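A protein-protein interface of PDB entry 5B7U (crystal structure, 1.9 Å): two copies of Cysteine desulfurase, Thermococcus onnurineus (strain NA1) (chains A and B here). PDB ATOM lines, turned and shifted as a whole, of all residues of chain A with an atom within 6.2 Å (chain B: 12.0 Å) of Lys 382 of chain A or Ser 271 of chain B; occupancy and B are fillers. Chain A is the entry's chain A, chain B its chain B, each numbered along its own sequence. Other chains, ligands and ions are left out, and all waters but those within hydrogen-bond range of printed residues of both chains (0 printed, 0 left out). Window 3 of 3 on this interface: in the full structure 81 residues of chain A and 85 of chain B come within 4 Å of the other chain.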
ATOM      1  N   LEU A 138      18.619 -15.122 -26.043  1.00  0.00           N
ATOM      2  CA  LEU A 138      19.486 -16.357 -26.223  1.00  0.00           C
ATOM      3  C   LEU A 138      19.827 -16.975 -24.921  1.00  0.00           C
ATOM      4  O   LEU A 138      19.518 -18.164 -24.687  1.00  0.00           O
ATOM      5  CB  LEU A 138      20.745 -16.001 -26.984  1.00  0.00           C
ATOM      6  CG  LEU A 138      21.743 -17.112 -27.293  1.00  0.00           C
ATOM      7  CD1 LEU A 138      21.087 -18.221 -28.039  1.00  0.00           C
ATOM      8  CD2 LEU A 138      22.857 -16.509 -28.138  1.00  0.00           C
ATOM      9  N   GLN A 142      19.582 -20.811 -23.461  1.00  0.00           N
ATOM     10  CA  GLN A 142      20.804 -21.581 -23.213  1.00  0.00           C
ATOM     11  C   GLN A 142      20.887 -22.112 -21.821  1.00  0.00           C
ATOM     12  O   GLN A 142      21.256 -23.304 -21.640  1.00  0.00           O
ATOM     13  CB  GLN A 142      22.075 -20.753 -23.483  1.00  0.00           C
ATOM     14  CG  GLN A 142      22.323 -20.446 -24.922  1.00  0.00           C
ATOM     15  CD  GLN A 142      23.480 -19.480 -25.120  1.00  0.00           C
ATOM     16  OE1 GLN A 142      23.696 -18.567 -24.317  1.00  0.00           O
ATOM     17  NE2 GLN A 142      24.185 -19.645 -26.206  1.00  0.00           N
ATOM     18  N   PHE A 154      19.152 -23.974 -33.936  1.00  0.00           N
ATOM     19  CA  PHE A 154      19.122 -22.676 -34.628  1.00  0.00           C
ATOM     20  C   PHE A 154      18.748 -22.811 -36.051  1.00  0.00           C
ATOM     21  O   PHE A 154      19.313 -23.653 -36.763  1.00  0.00           O
ATOM     22  CB  PHE A 154      20.493 -22.066 -34.519  1.00  0.00           C
ATOM     23  CG  PHE A 154      20.914 -21.840 -33.121  1.00  0.00           C
ATOM     24  CD1 PHE A 154      20.486 -20.695 -32.419  1.00  0.00           C
ATOM     25  CD2 PHE A 154      21.710 -22.761 -32.473  1.00  0.00           C
ATOM     26  CE1 PHE A 154      20.911 -20.482 -31.124  1.00  0.00           C
ATOM     27  CE2 PHE A 154      22.106 -22.588 -31.185  1.00  0.00           C
ATOM     28  CZ  PHE A 154      21.714 -21.436 -30.491  1.00  0.00           C
ATOM     29  N   ALA A 377      24.993  -8.861 -29.561  1.00  0.00           N
ATOM     30  CA  ALA A 377      24.742  -9.859 -30.555  1.00  0.00           C
ATOM     31  C   ALA A 377      26.040 -10.543 -31.059  1.00  0.00           C
ATOM     32  O   ALA A 377      26.290 -10.600 -32.211  1.00  0.00           O
ATOM     33  CB  ALA A 377      23.963  -9.251 -31.679  1.00  0.00           C
ATOM     34  N   LEU A 378      26.828 -11.055 -30.141  1.00  0.00           N
ATOM     35  CA  LEU A 378      28.102 -11.706 -30.466  1.00  0.00           C
ATOM     36  C   LEU A 378      27.993 -12.831 -31.480  1.00  0.00           C
ATOM     37  O   LEU A 378      28.820 -12.915 -32.339  1.00  0.00           O
ATOM     38  CB  LEU A 378      28.883 -12.131 -29.228  1.00  0.00           C
ATOM     39  CG  LEU A 378      29.716 -10.996 -28.611  1.00  0.00           C
ATOM     40  CD1 LEU A 378      30.082 -11.205 -27.127  1.00  0.00           C
ATOM     41  CD2 LEU A 378      30.986 -10.778 -29.432  1.00  0.00           C
ATOM     42  N   PRO A 379      26.938 -13.619 -31.437  1.00  0.00           N
ATOM     43  CA  PRO A 379      26.835 -14.661 -32.460  1.00  0.00           C
ATOM     44  C   PRO A 379      26.659 -14.138 -33.885  1.00  0.00           C
ATOM     45  O   PRO A 379      27.138 -14.765 -34.828  1.00  0.00           O
ATOM     46  CB  PRO A 379      25.632 -15.470 -31.993  1.00  0.00           C
ATOM     47  CG  PRO A 379      25.752 -15.391 -30.500  1.00  0.00           C
ATOM     48  CD  PRO A 379      26.050 -13.916 -30.290  1.00  0.00           C
ATOM     49  N   VAL A 380      25.977 -12.999 -34.050  1.00  0.00           N
ATOM     50  CA  VAL A 380      25.970 -12.323 -35.344  1.00  0.00           C
ATOM     51  C   VAL A 380      27.421 -11.970 -35.816  1.00  0.00           C
ATOM     52  O   VAL A 380      27.788 -12.221 -36.978  1.00  0.00           O
ATOM     53  CB  VAL A 380      25.082 -11.065 -35.360  1.00  0.00           C
ATOM     54  CG1 VAL A 380      25.197 -10.361 -36.686  1.00  0.00           C
ATOM     55  CG2 VAL A 380      23.631 -11.470 -35.132  1.00  0.00           C
ATOM     56  N   MET A 381      28.173 -11.351 -34.943  1.00  0.00           N
ATOM     57  CA  MET A 381      29.538 -10.876 -35.272  1.00  0.00           C
ATOM     58  C   MET A 381      30.406 -12.104 -35.651  1.00  0.00           C
ATOM     59  O   MET A 381      31.106 -12.108 -36.665  1.00  0.00           O
ATOM     60  CB  MET A 381      30.123 -10.107 -34.115  1.00  0.00           C
ATOM     61  CG  MET A 381      29.426  -8.776 -33.756  1.00  0.00           C
ATOM     62  SD  MET A 381      28.915  -7.861 -35.202  1.00  0.00           S
ATOM     63  CE  MET A 381      27.372  -7.092 -34.667  1.00  0.00           C
ATOM     64  N   LYS A 382      30.264 -13.169 -34.867  1.00  0.00           N
ATOM     65  CA  LYS A 382      31.043 -14.387 -35.062  1.00  0.00           C
ATOM     66  C   LYS A 382      30.673 -15.070 -36.344  1.00  0.00           C
ATOM     67  O   LYS A 382      31.581 -15.505 -37.074  1.00  0.00           O
ATOM     68  CB  LYS A 382      30.907 -15.306 -33.872  1.00  0.00           C
ATOM     69  CG  LYS A 382      31.623 -14.726 -32.683  1.00  0.00           C
ATOM     70  CD  LYS A 382      31.534 -15.613 -31.440  1.00  0.00           C
ATOM     71  CE  LYS A 382      32.038 -14.821 -30.262  1.00  0.00           C
ATOM     72  NZ  LYS A 382      32.147 -15.612 -28.998  1.00  0.00           N
ATOM     73  N   LYS A 383      29.378 -15.129 -36.660  1.00  0.00           N
ATOM     74  CA  LYS A 383      28.895 -15.663 -37.938  1.00  0.00           C
ATOM     75  C   LYS A 383      29.403 -14.889 -39.175  1.00  0.00           C
ATOM     76  O   LYS A 383      29.732 -15.482 -40.235  1.00  0.00           O
ATOM     77  CB  LYS A 383      27.361 -15.732 -37.952  1.00  0.00           C
ATOM     78  CG  LYS A 383      26.711 -16.263 -39.219  1.00  0.00           C
ATOM     79  CD  LYS A 383      25.188 -16.341 -39.057  1.00  0.00           C
ATOM     80  CE  LYS A 383      24.484 -16.688 -40.359  1.00  0.00           C
ATOM     81  NZ  LYS A 383      24.685 -18.112 -40.696  1.00  0.00           N
ATOM     82  N   LEU A 384      29.437 -13.574 -39.074  1.00  0.00           N
ATOM     83  CA  LEU A 384      29.962 -12.736 -40.149  1.00  0.00           C
ATOM     84  C   LEU A 384      31.486 -12.676 -40.175  1.00  0.00           C
ATOM     85  O   LEU A 384      32.048 -12.095 -41.090  1.00  0.00           O
ATOM     86  CB  LEU A 384      29.379 -11.299 -40.043  1.00  0.00           C
ATOM     87  CG  LEU A 384      27.994 -11.195 -40.707  1.00  0.00           C
ATOM     88  CD1 LEU A 384      27.010 -12.264 -40.237  1.00  0.00           C
ATOM     89  CD2 LEU A 384      27.341  -9.859 -40.517  1.00  0.00           C
ATOM     90  N   GLY A 385      32.150 -13.183 -39.143  1.00  0.00           N
ATOM     91  CA  GLY A 385      33.591 -13.131 -39.049  1.00  0.00           C
ATOM     92  C   GLY A 385      34.127 -11.734 -38.823  1.00  0.00           C
ATOM     93  O   GLY A 385      35.162 -11.396 -39.379  1.00  0.00           O
ATOM     94  N   ILE A 386      33.438 -10.911 -38.025  1.00  0.00           N
ATOM     95  CA  ILE A 386      33.847  -9.515 -37.761  1.00  0.00           C
ATOM     96  C   ILE A 386      33.846  -9.319 -36.265  1.00  0.00           C
ATOM     97  O   ILE A 386      33.335 -10.174 -35.550  1.00  0.00           O
ATOM     98  CB  ILE A 386      32.969  -8.520 -38.515  1.00  0.00           C
ATOM     99  CG1 ILE A 386      31.514  -8.566 -38.001  1.00  0.00           C
ATOM    100  CG2 ILE A 386      33.011  -8.822 -40.001  1.00  0.00           C
ATOM    101  CD1 ILE A 386      30.544  -7.594 -38.657  1.00  0.00           C
ATOM    102  N   ILE B 262      19.312 -12.912 -16.900  1.00  0.00           N
ATOM    103  CA  ILE B 262      20.540 -12.775 -17.666  1.00  0.00           C
ATOM    104  C   ILE B 262      20.258 -12.392 -19.086  1.00  0.00           C
ATOM    105  O   ILE B 262      19.211 -12.651 -19.638  1.00  0.00           O
ATOM    106  CB  ILE B 262      21.355 -14.104 -17.630  1.00  0.00           C
ATOM    107  CG1 ILE B 262      20.523 -15.292 -18.041  1.00  0.00           C
ATOM    108  CG2 ILE B 262      21.912 -14.364 -16.247  1.00  0.00           C
ATOM    109  CD1 ILE B 262      21.361 -16.566 -18.287  1.00  0.00           C
ATOM    110  N   GLY B 263      21.243 -11.803 -19.736  1.00  0.00           N
ATOM    111  CA  GLY B 263      21.046 -11.337 -21.058  1.00  0.00           C
ATOM    112  C   GLY B 263      21.948 -10.191 -21.384  1.00  0.00           C
ATOM    113  O   GLY B 263      23.132 -10.143 -20.949  1.00  0.00           O
ATOM    114  N   GLY B 264      21.403  -9.246 -22.153  1.00  0.00           N
ATOM    115  CA  GLY B 264      22.103  -7.987 -22.477  1.00  0.00           C
ATOM    116  C   GLY B 264      22.742  -7.319 -21.264  1.00  0.00           C
ATOM    117  O   GLY B 264      22.153  -7.214 -20.214  1.00  0.00           O
ATOM    118  N   THR B 266      24.989  -8.413 -19.158  1.00  0.00           N
ATOM    119  CA  THR B 266      25.512  -9.274 -18.101  1.00  0.00           C
ATOM    120  C   THR B 266      26.679 -10.220 -18.512  1.00  0.00           C
ATOM    121  O   THR B 266      27.075 -11.036 -17.745  1.00  0.00           O
ATOM    122  CB  THR B 266      24.382 -10.157 -17.506  1.00  0.00           C
ATOM    123  OG1 THR B 266      24.020 -11.196 -18.419  1.00  0.00           O
ATOM    124  CG2 THR B 266      23.156  -9.299 -17.151  1.00  0.00           C
ATOM    125  N   ILE B 267      27.165 -10.077 -19.732  1.00  0.00           N
ATOM    126  CA  ILE B 267      28.151 -10.970 -20.282  1.00  0.00           C
ATOM    127  C   ILE B 267      29.507 -10.434 -20.665  1.00  0.00           C
ATOM    128  O   ILE B 267      29.673  -9.284 -20.915  1.00  0.00           O
ATOM    129  CB  ILE B 267      27.649 -11.638 -21.581  1.00  0.00           C
ATOM    130  CG1 ILE B 267      27.501 -10.628 -22.693  1.00  0.00           C
ATOM    131  CG2 ILE B 267      26.360 -12.410 -21.376  1.00  0.00           C
ATOM    132  CD1 ILE B 267      28.761 -10.330 -23.463  1.00  0.00           C
ATOM    133  N   GLU B 268      30.454 -11.351 -20.707  1.00  0.00           N
ATOM    134  CA  GLU B 268      31.789 -11.069 -21.124  1.00  0.00           C
ATOM    135  C   GLU B 268      31.910 -11.665 -22.508  1.00  0.00           C
ATOM    136  O   GLU B 268      32.544 -11.110 -23.337  1.00  0.00           O
ATOM    137  CB  GLU B 268      32.806 -11.674 -20.200  1.00  0.00           C
ATOM    138  CG  GLU B 268      34.020 -10.826 -20.059  1.00  0.00           C
ATOM    139  CD  GLU B 268      34.882 -11.289 -18.927  1.00  0.00           C
ATOM    140  OE1 GLU B 268      34.866 -10.604 -17.904  1.00  0.00           O
ATOM    141  OE2 GLU B 268      35.524 -12.335 -19.064  1.00  0.00           O
ATOM    142  N   ASP B 269      31.283 -12.805 -22.726  1.00  0.00           N
ATOM    143  CA  ASP B 269      31.298 -13.445 -24.022  1.00  0.00           C
ATOM    144  C   ASP B 269      30.129 -14.419 -24.217  1.00  0.00           C
ATOM    145  O   ASP B 269      29.653 -15.023 -23.313  1.00  0.00           O
ATOM    146  CB  ASP B 269      32.646 -14.163 -24.273  1.00  0.00           C
ATOM    147  CG  ASP B 269      32.764 -14.754 -25.673  1.00  0.00           C
ATOM    148  OD1 ASP B 269      32.397 -14.162 -26.673  1.00  0.00           O
ATOM    149  OD2 ASP B 269      33.270 -15.861 -25.761  1.00  0.00           O
ATOM    150  N   VAL B 270      29.729 -14.534 -25.449  1.00  0.00           N
ATOM    151  CA  VAL B 270      28.673 -15.388 -25.873  1.00  0.00           C
ATOM    152  C   VAL B 270      28.937 -15.984 -27.241  1.00  0.00           C
ATOM    153  O   VAL B 270      29.513 -15.365 -28.103  1.00  0.00           O
ATOM    154  CB  VAL B 270      27.377 -14.580 -26.061  1.00  0.00           C
ATOM    155  CG1 VAL B 270      26.232 -15.452 -26.553  1.00  0.00           C
ATOM    156  CG2 VAL B 270      27.048 -13.791 -24.839  1.00  0.00           C
ATOM    157  N   SER B 271      28.427 -17.182 -27.418  1.00  0.00           N
ATOM    158  CA  SER B 271      28.478 -17.843 -28.669  1.00  0.00           C
ATOM    159  C   SER B 271      27.198 -18.681 -28.723  1.00  0.00           C
ATOM    160  O   SER B 271      26.551 -18.851 -27.743  1.00  0.00           O
ATOM    161  CB  SER B 271      29.734 -18.718 -28.771  1.00  0.00           C
ATOM    162  OG  SER B 271      29.669 -19.778 -27.878  1.00  0.00           O
ATOM    163  N   LEU B 272      26.865 -19.212 -29.869  1.00  0.00           N
ATOM    164  CA  LEU B 272      25.701 -20.035 -29.987  1.00  0.00           C
ATOM    165  C   LEU B 272      25.678 -21.182 -28.980  1.00  0.00           C
ATOM    166  O   LEU B 272      24.643 -21.632 -28.600  1.00  0.00           O
ATOM    167  CB  LEU B 272      25.671 -20.601 -31.367  1.00  0.00           C
ATOM    168  CG  LEU B 272      24.713 -19.983 -32.343  1.00  0.00           C
ATOM    169  CD1 LEU B 272      24.137 -18.639 -31.976  1.00  0.00           C
ATOM    170  CD2 LEU B 272      25.177 -20.066 -33.748  1.00  0.00           C
ATOM    171  N   ASP B 273      26.844 -21.667 -28.575  1.00  0.00           N
ATOM    172  CA  ASP B 273      26.900 -22.777 -27.658  1.00  0.00           C
ATOM    173  C   ASP B 273      27.140 -22.450 -26.216  1.00  0.00           C
ATOM    174  O   ASP B 273      27.340 -23.341 -25.464  1.00  0.00           O
ATOM    175  CB  ASP B 273      27.863 -23.866 -28.146  1.00  0.00           C
ATOM    176  CG  ASP B 273      29.236 -23.381 -28.337  1.00  0.00           C
ATOM    177  OD1 ASP B 273      29.546 -22.284 -27.870  1.00  0.00           O
ATOM    178  OD2 ASP B 273      30.044 -24.107 -28.938  1.00  0.00           O
ATOM    179  N   GLY B 274      27.106 -21.189 -25.819  1.00  0.00           N
ATOM    180  CA  GLY B 274      27.315 -20.862 -24.424  1.00  0.00           C
ATOM    181  C   GLY B 274      27.614 -19.425 -24.067  1.00  0.00           C
ATOM    182  O   GLY B 274      27.615 -18.581 -24.905  1.00  0.00           O
ATOM    183  N   TYR B 275      27.880 -19.173 -22.803  1.00  0.00           N
ATOM    184  CA  TYR B 275      28.129 -17.796 -22.394  1.00  0.00           C
ATOM    185  C   TYR B 275      28.975 -17.774 -21.191  1.00  0.00           C
ATOM    186  O   TYR B 275      29.004 -18.728 -20.467  1.00  0.00           O
ATOM    187  CB  TYR B 275      26.781 -17.061 -22.075  1.00  0.00           C
ATOM    188  CG  TYR B 275      25.981 -17.613 -20.910  1.00  0.00           C
ATOM    189  CD1 TYR B 275      26.174 -17.164 -19.627  1.00  0.00           C
ATOM    190  CD2 TYR B 275      25.027 -18.611 -21.128  1.00  0.00           C
ATOM    191  CE1 TYR B 275      25.469 -17.705 -18.584  1.00  0.00           C
ATOM    192  CE2 TYR B 275      24.306 -19.158 -20.098  1.00  0.00           C
ATOM    193  CZ  TYR B 275      24.526 -18.704 -18.835  1.00  0.00           C
ATOM    194  OH  TYR B 275      23.815 -19.236 -17.808  1.00  0.00           O
ATOM    195  N   LYS B 276      29.580 -16.626 -20.951  1.00  0.00           N
ATOM    196  CA  LYS B 276      30.306 -16.273 -19.749  1.00  0.00           C
ATOM    197  C   LYS B 276      29.863 -14.893 -19.195  1.00  0.00           C
ATOM    198  O   LYS B 276      29.901 -13.901 -19.895  1.00  0.00           O
ATOM    199  CB  LYS B 276      31.810 -16.196 -20.071  1.00  0.00           C
ATOM    200  CG  LYS B 276      32.622 -15.684 -18.890  1.00  0.00           C
ATOM    201  CD  LYS B 276      33.934 -16.416 -18.720  1.00  0.00           C
ATOM    202  CE  LYS B 276      34.438 -16.291 -17.290  1.00  0.00           C
ATOM    203  NZ  LYS B 276      35.055 -14.959 -17.100  1.00  0.00           N
ATOM    204  N   LEU B 277      29.497 -14.840 -17.940  1.00  0.00           N
ATOM    205  CA  LEU B 277      29.000 -13.590 -17.354  1.00  0.00           C
ATOM    206  C   LEU B 277      30.146 -12.660 -16.973  1.00  0.00           C
ATOM    207  O   LEU B 277      31.243 -13.105 -16.713  1.00  0.00           O
ATOM    208  CB  LEU B 277      28.109 -13.822 -16.127  1.00  0.00           C
ATOM    209  CG  LEU B 277      26.593 -14.118 -16.282  1.00  0.00           C
ATOM    210  CD1 LEU B 277      26.048 -14.256 -17.709  1.00  0.00           C
ATOM    211  CD2 LEU B 277      26.259 -15.297 -15.397  1.00  0.00           C
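Among the printed residues, merely in contact across the chains: Leu 138 of chain A with Val 270 of chain B (3.9 Å), Gln 142 of chain A with Tyr 275 of chain B (3.5 Å), Phe 154 of chain A with Leu 272 of chain B (3.5 Å), Leu 378 of chain A with Ile 267 of chain B (3.99 Å), Leu 378 of chain A with Asp 269 of chain B (3.8 Å), Leu 378 of chain A with Val 270 of chain B (3.5 Å), Pro 379 of chain A with Val 270 of chain B (3.98 Å), Pro 379 of chain A with Leu 272 of chain B (3.5 Å) and Lys 382 of chain A with Ser 271 of chain B (3.9 Å).
Printed residues of chain B that touch a printed residue of chain A: Ile 267, Asp 269, Val 270, Ser 271, Leu 272, Gly 274 and Tyr 275.
Among the printed residues, 14 pairs touch across the chains.
Among the printed residues, Asp or Glu carboxylates within 4 Å of a Lys or Arg side-chain nitrogen of the other chain: Lys 382 of chain A with Asp 269 of chain B.
O of Ser 271 of chain B lies within hydrogen-bond range of NE2 of Gln 142 of chain A, at 2.9 Å.
The backbone carbonyl oxygen (O) of Leu 272 of chain B sits at hydrogen-bond distance from the side-chain amide nitrogen (NE2) of Gln 142 of chain A, 3.1 Å away.
The side-chain amide nitrogen of Gln 142 of chain A sits close to the backbone NH of Gly 274 of chain B (3.3 Å).
The side-chain carboxylate of Asp 269 of chain B lies within salt-bridge range of the side-chain amino group of Lys 382 of chain A (2.8 Å).
The side-chain amino group of Lys 382 of chain A lies within hydrogen-bond range of the backbone carbonyl oxygen of Val 270 of chain B (2.8 Å).
Of chain B, only Asp 269, Val 270 and Ser 271 come within 4 Å of Lys 382 of chain A.
Of the printed residues of chain A, Ser 271 of chain B touches Gln 142 and Lys 382.
No residue of chain B comes within 4 Å of Val 380 of chain A.
No residue of chain B comes within 4 Å of Leu 384 of chain A.
No residue of chain B comes within 4 Å of Gly 385 of chain A.
Ile 386 of chain A touches none of the printed residues of chain B.
Printed residues of chain A within 4 Å of Val 270 of chain B: Leu 138, Leu 378, Pro 379 and Lys 382.
Of the printed residues of chain B, Phe 154 of chain A touches Leu 272.
Glu 268 of chain B touches none of the printed residues of chain A.
Ala 377 of chain A touches none of the printed residues of chain B.
The nearest printed residue of chain A that does not touch Ser 271 of chain B is Pro 379 of chain A (4.01 Å).
The nearest printed residue of chain B that does not touch Gln 142 of chain A is Asp 273 of chain B (4.1 Å).
No position is printed for both chains.
The backbone carbonyl oxygen (O) of Asp 269 of chain B lies within hydrogen-bond range of the backbone NH (N) of Lys 276 of chain B, at 2.9 Å.
The side-chain carboxylate (OD1) of Asp 273 of chain B sits at hydrogen-bond distance from the side-chain hydroxyl (OG) of Ser 271 of chain B (2.5 Å).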
